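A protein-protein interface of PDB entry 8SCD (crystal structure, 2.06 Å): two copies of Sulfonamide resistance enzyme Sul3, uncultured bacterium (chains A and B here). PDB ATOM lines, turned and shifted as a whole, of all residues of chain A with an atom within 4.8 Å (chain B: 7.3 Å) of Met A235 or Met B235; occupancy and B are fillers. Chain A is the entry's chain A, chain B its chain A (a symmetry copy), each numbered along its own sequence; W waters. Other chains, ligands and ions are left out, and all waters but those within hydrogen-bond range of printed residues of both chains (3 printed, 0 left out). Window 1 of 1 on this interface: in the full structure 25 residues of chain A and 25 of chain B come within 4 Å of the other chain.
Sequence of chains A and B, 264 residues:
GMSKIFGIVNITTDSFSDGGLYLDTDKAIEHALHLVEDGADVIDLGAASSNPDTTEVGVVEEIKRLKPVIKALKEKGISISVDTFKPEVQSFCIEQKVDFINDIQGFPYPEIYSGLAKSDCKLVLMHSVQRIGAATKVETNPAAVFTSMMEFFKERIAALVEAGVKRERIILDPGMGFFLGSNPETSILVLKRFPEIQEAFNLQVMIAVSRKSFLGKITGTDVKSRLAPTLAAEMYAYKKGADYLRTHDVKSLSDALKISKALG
The side-chain hydroxyl (OH) of Tyr A236 is in hydrogen-bond range of the backbone carbonyl oxygen (O) of Leu B263 (3.5 Å).
SD of Met A235 lies within hydrogen-bond range of OG of Ser A260.
The backbone carbonyl oxygen of Ala B256 lies within hydrogen-bond range of the side-chain hydroxyl of Ser B260 (2.8 Å).
SD of Met B235 lies within hydrogen-bond range of OG of Ser B260 (3.1 Å).
The backbone carbonyl oxygen of Ala A256 lies within hydrogen-bond range of the side-chain hydroxyl of Ser A260.
Among the printed residues, merely in contact across the chains: Met A235 with Met B235, Ala A232 with Ala B256, Ala A256 with Ala B232, Ala A232 with Met B235, Met A235 with Ala B232, Ala A232 with Ile B259, Leu A231 with Ala B228 and Ala A233 with Ile B259.
Printed residues of chain B within 4 Å of Leu A231: Ala B228 (3.7 Å).
Printed residues of chain B within 4 Å of Ala A232: Met B235 (3.6 Å), Ala B256 (3.6 Å) and Ile B259 (3.7 Å).
Of the printed residues of chain B, Ala A233 touches Ile B259 (3.8 Å).
Of chain B, only Ala B232 and Met B235 come within 4 Å of Met A235.
Printed residues of chain B within 4 Å of Ala A256: Ala B232 (3.6 Å).
Met B235 touches just these residues of chain A: Ala A232 and Met A235.
Tyr B238 touches none of the printed residues of chain A.
The nearest residue of chain B that does not touch Met A235 is Leu B231 (4.7 Å).
The nearest residue of chain A that does not touch Met B235 is Leu A231 (4.7 Å).
Of the 12 printed residues of chain A, 6 touch a printed residue of chain B.
Among the printed residues, no Asp or Glu carboxylate lies within 4 Å of a Lys or Arg side-chain nitrogen of the other chain.
Ala A232 touches Met B235, and with the chains exchanged Met A235 touches Ala B232.
Ala A232 touches Ala B256, and with the chains exchanged Ala A256 touches Ala B232.
Met A235 touches its own counterpart, Met B235.
Positions printed for both chains: 231, 232, 233, 234, 235, 236, 237, 238, 239, 256, 257 and 260.
Water W2 bridges OH of Tyr A236 (2.6 Å) and O of Leu B263 (2.9 Å).
Water W1 lies within hydrogen-bond range of O of Ala A232 (2.7 Å) and OG of Ser B260 (3.1 Å).
Water W3 lies within hydrogen-bond range of the backbone carbonyl oxygen (O) of Ala B232 (2.7 Å) and the side-chain hydroxyl (OG) of Ser A260 (3.1 Å).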
ATOM      1  N   LEU A 231      -3.710   7.648 -13.404  1.00  0.00           N
ATOM      2  CA  LEU A 231      -4.436   8.748 -14.033  1.00  0.00           C
ATOM      3  C   LEU A 231      -4.354  10.020 -13.201  1.00  0.00           C
ATOM      4  O   LEU A 231      -4.274  11.125 -13.750  1.00  0.00           O
ATOM      5  CB  LEU A 231      -5.897   8.362 -14.255  1.00  0.00           C
ATOM      6  CG  LEU A 231      -6.190   7.393 -15.397  1.00  0.00           C
ATOM      7  CD1 LEU A 231      -7.659   7.005 -15.389  1.00  0.00           C
ATOM      8  CD2 LEU A 231      -5.803   8.024 -16.724  1.00  0.00           C
ATOM      9  N   ALA A 232      -4.395   9.888 -11.873  1.00  0.00           N
ATOM     10  CA  ALA A 232      -4.287  11.066 -11.020  1.00  0.00           C
ATOM     11  C   ALA A 232      -2.942  11.756 -11.208  1.00  0.00           C
ATOM     12  O   ALA A 232      -2.874  12.987 -11.298  1.00  0.00           O
ATOM     13  CB  ALA A 232      -4.497  10.675  -9.558  1.00  0.00           C
ATOM     14  N   ALA A 233      -1.862  10.976 -11.294  1.00  0.00           N
ATOM     15  CA  ALA A 233      -0.541  11.566 -11.481  1.00  0.00           C
ATOM     16  C   ALA A 233      -0.343  12.066 -12.906  1.00  0.00           C
ATOM     17  O   ALA A 233       0.354  13.064 -13.118  1.00  0.00           O
ATOM     18  CB  ALA A 233       0.545  10.553 -11.118  1.00  0.00           C
ATOM     19  N   GLU A 234      -0.949  11.398 -13.890  1.00  0.00           N
ATOM     20  CA  GLU A 234      -0.758  11.805 -15.278  1.00  0.00           C
ATOM     21  C   GLU A 234      -1.460  13.124 -15.577  1.00  0.00           C
ATOM     22  O   GLU A 234      -0.906  13.977 -16.282  1.00  0.00           O
ATOM     23  CB  GLU A 234      -1.238  10.702 -16.220  1.00  0.00           C
ATOM     24  CG  GLU A 234      -0.263   9.546 -16.322  1.00  0.00           C
ATOM     25  CD  GLU A 234      -0.797   8.383 -17.128  1.00  0.00           C
ATOM     26  OE1 GLU A 234      -2.028   8.283 -17.306  1.00  0.00           O
ATOM     27  OE2 GLU A 234       0.024   7.554 -17.569  1.00  0.00           O
ATOM     28  N   MET A 235      -2.673  13.324 -15.057  1.00  0.00           N
ATOM     29  CA  MET A 235      -3.329  14.608 -15.280  1.00  0.00           C
ATOM     30  C   MET A 235      -2.771  15.724 -14.413  1.00  0.00           C
ATOM     31  O   MET A 235      -2.892  16.893 -14.793  1.00  0.00           O
ATOM     32  CB  MET A 235      -4.840  14.500 -15.078  1.00  0.00           C
ATOM     33  CG  MET A 235      -5.551  13.951 -16.306  1.00  0.00           C
ATOM     34  SD  MET A 235      -7.271  13.517 -16.040  1.00  0.00           S
ATOM     35  CE  MET A 235      -7.304  13.317 -14.275  1.00  0.00           C
ATOM     36  N   TYR A 236      -2.169  15.408 -13.268  1.00  0.00           N
ATOM     37  CA  TYR A 236      -1.381  16.422 -12.578  1.00  0.00           C
ATOM     38  C   TYR A 236      -0.229  16.883 -13.461  1.00  0.00           C
ATOM     39  O   TYR A 236       0.014  18.086 -13.611  1.00  0.00           O
ATOM     40  CB  TYR A 236      -0.861  15.886 -11.246  1.00  0.00           C
ATOM     41  CG  TYR A 236       0.069  16.848 -10.532  1.00  0.00           C
ATOM     42  CD1 TYR A 236       1.441  16.827 -10.767  1.00  0.00           C
ATOM     43  CD2 TYR A 236      -0.427  17.781  -9.631  1.00  0.00           C
ATOM     44  CE1 TYR A 236       2.289  17.708 -10.122  1.00  0.00           C
ATOM     45  CE2 TYR A 236       0.414  18.663  -8.981  1.00  0.00           C
ATOM     46  CZ  TYR A 236       1.769  18.622  -9.230  1.00  0.00           C
ATOM     47  OH  TYR A 236       2.604  19.501  -8.581  1.00  0.00           O
ATOM     48  N   ALA A 237       0.483  15.931 -14.069  1.00  0.00           N
ATOM     49  CA  ALA A 237       1.603  16.279 -14.937  1.00  0.00           C
ATOM     50  C   ALA A 237       1.131  17.039 -16.169  1.00  0.00           C
ATOM     51  O   ALA A 237       1.797  17.979 -16.619  1.00  0.00           O
ATOM     52  CB  ALA A 237       2.366  15.019 -15.341  1.00  0.00           C
ATOM     53  N   TYR A 238      -0.014  16.645 -16.731  1.00  0.00           N
ATOM     54  CA  TYR A 238      -0.559  17.364 -17.878  1.00  0.00           C
ATOM     55  C   TYR A 238      -0.931  18.793 -17.500  1.00  0.00           C
ATOM     56  O   TYR A 238      -0.610  19.742 -18.225  1.00  0.00           O
ATOM     57  CB  TYR A 238      -1.773  16.620 -18.436  1.00  0.00           C
ATOM     58  CG  TYR A 238      -2.765  17.515 -19.147  1.00  0.00           C
ATOM     59  CD1 TYR A 238      -2.463  18.080 -20.379  1.00  0.00           C
ATOM     60  CD2 TYR A 238      -4.005  17.793 -18.585  1.00  0.00           C
ATOM     61  CE1 TYR A 238      -3.367  18.900 -21.033  1.00  0.00           C
ATOM     62  CE2 TYR A 238      -4.916  18.611 -19.232  1.00  0.00           C
ATOM     63  CZ  TYR A 238      -4.591  19.162 -20.454  1.00  0.00           C
ATOM     64  OH  TYR A 238      -5.495  19.976 -21.100  1.00  0.00           O
ATOM     65  N   LYS A 239      -1.609  18.964 -16.361  1.00  0.00           N
ATOM     66  CA  LYS A 239      -1.995  20.304 -15.929  1.00  0.00           C
ATOM     67  C   LYS A 239      -0.777  21.169 -15.639  1.00  0.00           C
ATOM     68  O   LYS A 239      -0.839  22.395 -15.782  1.00  0.00           O
ATOM     69  CB  LYS A 239      -2.896  20.225 -14.695  1.00  0.00           C
ATOM     70  CG  LYS A 239      -4.308  19.734 -14.976  1.00  0.00           C
ATOM     71  CD  LYS A 239      -4.927  20.452 -16.166  1.00  0.00           C
ATOM     72  CE  LYS A 239      -5.675  21.702 -15.734  1.00  0.00           C
ATOM     73  NZ  LYS A 239      -6.304  22.400 -16.890  1.00  0.00           N
ATOM     74  N   ALA A 256      -9.328  10.793 -20.278  1.00  0.00           N
ATOM     75  CA  ALA A 256      -9.156  11.684 -19.137  1.00  0.00           C
ATOM     76  C   ALA A 256      -8.671  13.062 -19.576  1.00  0.00           C
ATOM     77  O   ALA A 256      -9.111  14.081 -19.033  1.00  0.00           O
ATOM     78  CB  ALA A 256      -8.187  11.057 -18.138  1.00  0.00           C
ATOM     79  N   LEU A 257      -7.764  13.112 -20.556  1.00  0.00           N
ATOM     80  CA  LEU A 257      -7.300  14.399 -21.066  1.00  0.00           C
ATOM     81  C   LEU A 257      -8.410  15.154 -21.785  1.00  0.00           C
ATOM     82  O   LEU A 257      -8.442  16.389 -21.748  1.00  0.00           O
ATOM     83  CB  LEU A 257      -6.107  14.199 -22.005  1.00  0.00           C
ATOM     84  CG  LEU A 257      -4.803  13.688 -21.387  1.00  0.00           C
ATOM     85  CD1 LEU A 257      -3.732  13.534 -22.454  1.00  0.00           C
ATOM     86  CD2 LEU A 257      -4.327  14.610 -20.278  1.00  0.00           C
ATOM     87  N   SER A 260     -10.480  16.745 -18.994  1.00  0.00           N
ATOM     88  CA  SER A 260      -9.739  17.840 -18.373  1.00  0.00           C
ATOM     89  C   SER A 260      -9.661  19.048 -19.297  1.00  0.00           C
ATOM     90  O   SER A 260      -9.721  20.195 -18.837  1.00  0.00           O
ATOM     91  CB  SER A 260      -8.336  17.372 -17.987  1.00  0.00           C
ATOM     92  OG  SER A 260      -8.384  16.143 -17.282  1.00  0.00           O
ATOM     93  N   VAL B 209     -21.041  13.122 -10.628  1.00  0.00           N
ATOM     94  CA  VAL B 209     -20.791  12.945 -12.055  1.00  0.00           C
ATOM     95  C   VAL B 209     -20.635  11.489 -12.459  1.00  0.00           C
ATOM     96  O   VAL B 209     -20.652  11.199 -13.667  1.00  0.00           O
ATOM     97  CB  VAL B 209     -19.546  13.737 -12.513  1.00  0.00           C
ATOM     98  CG1 VAL B 209     -19.686  15.206 -12.167  1.00  0.00           C
ATOM     99  CG2 VAL B 209     -18.288  13.149 -11.888  1.00  0.00           C
ATOM    100  N   ALA B 228     -12.259   6.272 -16.400  1.00  0.00           N
ATOM    101  CA  ALA B 228     -11.290   7.335 -16.653  1.00  0.00           C
ATOM    102  C   ALA B 228     -11.938   8.706 -16.813  1.00  0.00           C
ATOM    103  O   ALA B 228     -11.464   9.662 -16.174  1.00  0.00           O
ATOM    104  CB  ALA B 228     -10.431   6.971 -17.870  1.00  0.00           C
ATOM    105  N   PRO B 229     -12.989   8.892 -17.623  1.00  0.00           N
ATOM    106  CA  PRO B 229     -13.628  10.217 -17.655  1.00  0.00           C
ATOM    107  C   PRO B 229     -14.290  10.587 -16.343  1.00  0.00           C
ATOM    108  O   PRO B 229     -14.340  11.776 -16.004  1.00  0.00           O
ATOM    109  CB  PRO B 229     -14.651  10.095 -18.794  1.00  0.00           C
ATOM    110  CG  PRO B 229     -14.902   8.647 -18.928  1.00  0.00           C
ATOM    111  CD  PRO B 229     -13.603   7.975 -18.602  1.00  0.00           C
ATOM    112  N   THR B 230     -14.800   9.607 -15.592  1.00  0.00           N
ATOM    113  CA  THR B 230     -15.358   9.896 -14.275  1.00  0.00           C
ATOM    114  C   THR B 230     -14.288  10.439 -13.338  1.00  0.00           C
ATOM    115  O   THR B 230     -14.483  11.471 -12.684  1.00  0.00           O
ATOM    116  CB  THR B 230     -16.002   8.639 -13.686  1.00  0.00           C
ATOM    117  OG1 THR B 230     -17.218   8.346 -14.388  1.00  0.00           O
ATOM    118  CG2 THR B 230     -16.314   8.836 -12.217  1.00  0.00           C
ATOM    119  N   LEU B 231     -13.139   9.757 -13.267  1.00  0.00           N
ATOM    120  CA  LEU B 231     -12.064  10.196 -12.380  1.00  0.00           C
ATOM    121  C   LEU B 231     -11.547  11.574 -12.767  1.00  0.00           C
ATOM    122  O   LEU B 231     -11.196  12.378 -11.896  1.00  0.00           O
ATOM    123  CB  LEU B 231     -10.919   9.185 -12.392  1.00  0.00           C
ATOM    124  CG  LEU B 231     -11.141   7.880 -11.633  1.00  0.00           C
ATOM    125  CD1 LEU B 231      -9.973   6.936 -11.865  1.00  0.00           C
ATOM    126  CD2 LEU B 231     -11.320   8.167 -10.152  1.00  0.00           C
ATOM    127  N   ALA B 232     -11.472  11.858 -14.069  1.00  0.00           N
ATOM    128  CA  ALA B 232     -11.016  13.173 -14.503  1.00  0.00           C
ATOM    129  C   ALA B 232     -11.957  14.267 -14.014  1.00  0.00           C
ATOM    130  O   ALA B 232     -11.509  15.317 -13.541  1.00  0.00           O
ATOM    131  CB  ALA B 232     -10.887  13.208 -16.024  1.00  0.00           C
ATOM    132  N   ALA B 233     -13.267  14.027 -14.100  1.00  0.00           N
ATOM    133  CA  ALA B 233     -14.229  15.026 -13.646  1.00  0.00           C
ATOM    134  C   ALA B 233     -14.300  15.092 -12.126  1.00  0.00           C
ATOM    135  O   ALA B 233     -14.527  16.169 -11.565  1.00  0.00           O
ATOM    136  CB  ALA B 233     -15.612  14.730 -14.229  1.00  0.00           C
ATOM    137  N   GLU B 234     -14.100  13.962 -11.444  1.00  0.00           N
ATOM    138  CA  GLU B 234     -14.201  13.957  -9.989  1.00  0.00           C
ATOM    139  C   GLU B 234     -13.033  14.694  -9.343  1.00  0.00           C
ATOM    140  O   GLU B 234     -13.227  15.434  -8.372  1.00  0.00           O
ATOM    141  CB  GLU B 234     -14.294  12.522  -9.473  1.00  0.00           C
ATOM    142  CG  GLU B 234     -15.669  11.913  -9.668  1.00  0.00           C
ATOM    143  CD  GLU B 234     -15.729  10.445  -9.304  1.00  0.00           C
ATOM    144  OE1 GLU B 234     -14.669   9.789  -9.253  1.00  0.00           O
ATOM    145  OE2 GLU B 234     -16.851   9.945  -9.087  1.00  0.00           O
ATOM    146  N   MET B 235     -11.814  14.519  -9.859  1.00  0.00           N
ATOM    147  CA  MET B 235     -10.698  15.269  -9.295  1.00  0.00           C
ATOM    148  C   MET B 235     -10.675  16.724  -9.730  1.00  0.00           C
ATOM    149  O   MET B 235     -10.102  17.553  -9.014  1.00  0.00           O
ATOM    150  CB  MET B 235      -9.362  14.606  -9.626  1.00  0.00           C
ATOM    151  CG  MET B 235      -9.034  13.458  -8.684  1.00  0.00           C
ATOM    152  SD  MET B 235      -7.641  12.449  -9.192  1.00  0.00           S
ATOM    153  CE  MET B 235      -7.570  12.815 -10.929  1.00  0.00           C
ATOM    154  N   TYR B 236     -11.272  17.064 -10.871  1.00  0.00           N
ATOM    155  CA  TYR B 236     -11.510  18.474 -11.153  1.00  0.00           C
ATOM    156  C   TYR B 236     -12.423  19.075 -10.092  1.00  0.00           C
ATOM    157  O   TYR B 236     -12.148  20.156  -9.558  1.00  0.00           O
ATOM    158  CB  TYR B 236     -12.112  18.650 -12.546  1.00  0.00           C
ATOM    159  CG  TYR B 236     -12.501  20.082 -12.857  1.00  0.00           C
ATOM    160  CD1 TYR B 236     -13.768  20.566 -12.544  1.00  0.00           C
ATOM    161  CD2 TYR B 236     -11.597  20.950 -13.455  1.00  0.00           C
ATOM    162  CE1 TYR B 236     -14.121  21.873 -12.821  1.00  0.00           C
ATOM    163  CE2 TYR B 236     -11.943  22.257 -13.738  1.00  0.00           C
ATOM    164  CZ  TYR B 236     -13.204  22.714 -13.419  1.00  0.00           C
ATOM    165  OH  TYR B 236     -13.546  24.014 -13.701  1.00  0.00           O
ATOM    166  N   ALA B 237     -13.509  18.373  -9.761  1.00  0.00           N
ATOM    167  CA  ALA B 237     -14.438  18.868  -8.752  1.00  0.00           C
ATOM    168  C   ALA B 237     -13.779  18.934  -7.381  1.00  0.00           C
ATOM    169  O   ALA B 237     -14.020  19.875  -6.615  1.00  0.00           O
ATOM    170  CB  ALA B 237     -15.685  17.987  -8.708  1.00  0.00           C
ATOM    171  N   TYR B 238     -12.948  17.944  -7.052  1.00  0.00           N
ATOM    172  CA  TYR B 238     -12.233  17.971  -5.779  1.00  0.00           C
ATOM    173  C   TYR B 238     -11.272  19.152  -5.719  1.00  0.00           C
ATOM    174  O   TYR B 238     -11.215  19.870  -4.714  1.00  0.00           O
ATOM    175  CB  TYR B 238     -11.485  16.653  -5.568  1.00  0.00           C
ATOM    176  CG  TYR B 238     -10.263  16.780  -4.686  1.00  0.00           C
ATOM    177  CD1 TYR B 238     -10.386  17.005  -3.320  1.00  0.00           C
ATOM    178  CD2 TYR B 238      -8.985  16.673  -5.218  1.00  0.00           C
ATOM    179  CE1 TYR B 238      -9.269  17.121  -2.509  1.00  0.00           C
ATOM    180  CE2 TYR B 238      -7.862  16.787  -4.415  1.00  0.00           C
ATOM    181  CZ  TYR B 238      -8.012  17.012  -3.062  1.00  0.00           C
ATOM    182  OH  TYR B 238      -6.898  17.126  -2.261  1.00  0.00           O
ATOM    183  N   LYS B 239     -10.506  19.369  -6.793  1.00  0.00           N
ATOM    184  CA  LYS B 239      -9.565  20.484  -6.811  1.00  0.00           C
ATOM    185  C   LYS B 239     -10.284  21.822  -6.731  1.00  0.00           C
ATOM    186  O   LYS B 239      -9.724  22.796  -6.218  1.00  0.00           O
ATOM    187  CB  LYS B 239      -8.695  20.422  -8.069  1.00  0.00           C
ATOM    188  CG  LYS B 239      -7.642  19.324  -8.055  1.00  0.00           C
ATOM    189  CD  LYS B 239      -6.865  19.307  -6.748  1.00  0.00           C
ATOM    190  CE  LYS B 239      -5.633  20.194  -6.820  1.00  0.00           C
ATOM    191  NZ  LYS B 239      -4.853  20.166  -5.552  1.00  0.00           N
ATOM    192  N   LYS B 240     -11.519  21.892  -7.228  1.00  0.00           N
ATOM    193  CA  LYS B 240     -12.297  23.121  -7.169  1.00  0.00           C
ATOM    194  C   LYS B 240     -13.017  23.306  -5.840  1.00  0.00           C
ATOM    195  O   LYS B 240     -13.671  24.337  -5.648  1.00  0.00           O
ATOM    196  CB  LYS B 240     -13.311  23.157  -8.317  1.00  0.00           C
ATOM    197  CG  LYS B 240     -12.689  23.421  -9.680  1.00  0.00           C
ATOM    198  CD  LYS B 240     -11.875  24.706  -9.676  1.00  0.00           C
ATOM    199  CE  LYS B 240     -11.358  25.038 -11.068  1.00  0.00           C
ATOM    200  NZ  LYS B 240      -9.873  24.970 -11.144  1.00  0.00           N
ATOM    201  N   GLY B 241     -12.917  22.347  -4.927  1.00  0.00           N
ATOM    202  CA  GLY B 241     -13.473  22.482  -3.602  1.00  0.00           C
ATOM    203  C   GLY B 241     -14.828  21.856  -3.358  1.00  0.00           C
ATOM    204  O   GLY B 241     -15.548  22.320  -2.468  1.00  0.00           O
ATOM    205  N   LEU B 245     -18.546  14.101  -2.917  1.00  0.00           N
ATOM    206  CA  LEU B 245     -18.516  13.452  -4.219  1.00  0.00           C
ATOM    207  C   LEU B 245     -19.295  12.152  -4.123  1.00  0.00           C
ATOM    208  O   LEU B 245     -19.011  11.315  -3.259  1.00  0.00           O
ATOM    209  CB  LEU B 245     -17.078  13.187  -4.681  1.00  0.00           C
ATOM    210  CG  LEU B 245     -16.258  14.419  -5.070  1.00  0.00           C
ATOM    211  CD1 LEU B 245     -14.819  14.034  -5.385  1.00  0.00           C
ATOM    212  CD2 LEU B 245     -16.896  15.137  -6.249  1.00  0.00           C
ATOM    213  N   SER B 252     -11.314   3.619  -6.535  1.00  0.00           N
ATOM    214  CA  SER B 252     -10.562   4.384  -7.525  1.00  0.00           C
ATOM    215  C   SER B 252     -10.534   5.866  -7.175  1.00  0.00           C
ATOM    216  O   SER B 252      -9.494   6.521  -7.307  1.00  0.00           O
ATOM    217  CB  SER B 252     -11.156   4.178  -8.917  1.00  0.00           C
ATOM    218  OG  SER B 252     -10.874   2.880  -9.408  1.00  0.00           O
ATOM    219  N   LEU B 253     -11.667   6.416  -6.732  1.00  0.00           N
ATOM    220  CA  LEU B 253     -11.695   7.821  -6.342  1.00  0.00           C
ATOM    221  C   LEU B 253     -10.799   8.072  -5.136  1.00  0.00           C
ATOM    222  O   LEU B 253     -10.045   9.051  -5.108  1.00  0.00           O
ATOM    223  CB  LEU B 253     -13.129   8.258  -6.047  1.00  0.00           C
ATOM    224  CG  LEU B 253     -13.306   9.698  -5.562  1.00  0.00           C
ATOM    225  CD1 LEU B 253     -12.669  10.679  -6.536  1.00  0.00           C
ATOM    226  CD2 LEU B 253     -14.781  10.018  -5.360  1.00  0.00           C
ATOM    227  N   ASP B 255      -8.139   6.316  -4.092  1.00  0.00           N
ATOM    228  CA  ASP B 255      -6.743   6.230  -4.509  1.00  0.00           C
ATOM    229  C   ASP B 255      -6.333   7.462  -5.301  1.00  0.00           C
ATOM    230  O   ASP B 255      -5.223   7.983  -5.129  1.00  0.00           O
ATOM    231  CB  ASP B 255      -6.521   4.966  -5.342  1.00  0.00           C
ATOM    232  CG  ASP B 255      -6.562   3.703  -4.508  1.00  0.00           C
ATOM    233  OD1 ASP B 255      -6.572   3.806  -3.261  1.00  0.00           O
ATOM    234  OD2 ASP B 255      -6.589   2.606  -5.101  1.00  0.00           O
ATOM    235  N   ALA B 256      -7.219   7.944  -6.170  1.00  0.00           N
ATOM    236  CA  ALA B 256      -6.921   9.132  -6.961  1.00  0.00           C
ATOM    237  C   ALA B 256      -6.813  10.373  -6.082  1.00  0.00           C
ATOM    238  O   ALA B 256      -5.950  11.228  -6.310  1.00  0.00           O
ATOM    239  CB  ALA B 256      -7.991   9.314  -8.035  1.00  0.00           C
ATOM    240  N   LEU B 257      -7.682  10.491  -5.073  1.00  0.00           N
ATOM    241  CA  LEU B 257      -7.599  11.624  -4.157  1.00  0.00           C
ATOM    242  C   LEU B 257      -6.328  11.578  -3.318  1.00  0.00           C
ATOM    243  O   LEU B 257      -5.780  12.630  -2.971  1.00  0.00           O
ATOM    244  CB  LEU B 257      -8.829  11.662  -3.245  1.00  0.00           C
ATOM    245  CG  LEU B 257     -10.180  11.965  -3.897  1.00  0.00           C
ATOM    246  CD1 LEU B 257     -11.289  11.949  -2.860  1.00  0.00           C
ATOM    247  CD2 LEU B 257     -10.146  13.296  -4.628  1.00  0.00           C
ATOM    248  N   LYS B 258      -5.849  10.379  -2.981  1.00  0.00           N
ATOM    249  CA  LYS B 258      -4.610  10.269  -2.216  1.00  0.00           C
ATOM    250  C   LYS B 258      -3.419  10.760  -3.027  1.00  0.00           C
ATOM    251  O   LYS B 258      -2.532  11.438  -2.492  1.00  0.00           O
ATOM    252  CB  LYS B 258      -4.393   8.824  -1.768  1.00  0.00           C
ATOM    253  CG  LYS B 258      -5.244   8.403  -0.586  1.00  0.00           C
ATOM    254  CD  LYS B 258      -4.847   7.020  -0.093  1.00  0.00           C
ATOM    255  CE  LYS B 258      -6.062   6.213   0.334  1.00  0.00           C
ATOM    256  NZ  LYS B 258      -5.736   4.770   0.494  1.00  0.00           N
ATOM    257  N   ILE B 259      -3.379  10.428  -4.319  1.00  0.00           N
ATOM    258  CA  ILE B 259      -2.304  10.910  -5.180  1.00  0.00           C
ATOM    259  C   ILE B 259      -2.389  12.423  -5.338  1.00  0.00           C
ATOM    260  O   ILE B 259      -1.387  13.136  -5.208  1.00  0.00           O
ATOM    261  CB  ILE B 259      -2.346  10.198  -6.544  1.00  0.00           C
ATOM    262  CG1 ILE B 259      -2.000   8.716  -6.389  1.00  0.00           C
ATOM    263  CG2 ILE B 259      -1.394  10.866  -7.526  1.00  0.00           C
ATOM    264  CD1 ILE B 259      -0.599   8.464  -5.868  1.00  0.00           C
ATOM    265  N   SER B 260      -3.592  12.937  -5.614  1.00  0.00           N
ATOM    266  CA  SER B 260      -3.760  14.375  -5.808  1.00  0.00           C
ATOM    267  C   SER B 260      -3.389  15.151  -4.552  1.00  0.00           C
ATOM    268  O   SER B 260      -2.821  16.246  -4.634  1.00  0.00           O
ATOM    269  CB  SER B 260      -5.199  14.684  -6.222  1.00  0.00           C
ATOM    270  OG  SER B 260      -5.620  13.836  -7.275  1.00  0.00           O
ATOM    271  N   LEU B 263       0.450  15.301  -4.269  1.00  0.00           N
ATOM    272  CA  LEU B 263       1.101  16.143  -5.265  1.00  0.00           C
ATOM    273  C   LEU B 263       0.751  17.616  -5.119  1.00  0.00           C
ATOM    274  O   LEU B 263       1.586  18.476  -5.429  1.00  0.00           O
ATOM    275  CB  LEU B 263       0.735  15.672  -6.675  1.00  0.00           C
ATOM    276  CG  LEU B 263       1.241  14.283  -7.063  1.00  0.00           C
ATOM    277  CD1 LEU B 263       0.810  13.931  -8.478  1.00  0.00           C
ATOM    278  CD2 LEU B 263       2.753  14.205  -6.919  1.00  0.00           C
HETATM  279  O   HOH W   1      -4.635  14.728 -10.119  1.00  0.00           O
HETATM  280  O   HOH W   2       1.837  21.034  -6.672  1.00  0.00           O
HETATM  281  O   HOH W   3      -9.102  16.431 -14.240  1.00  0.00           O
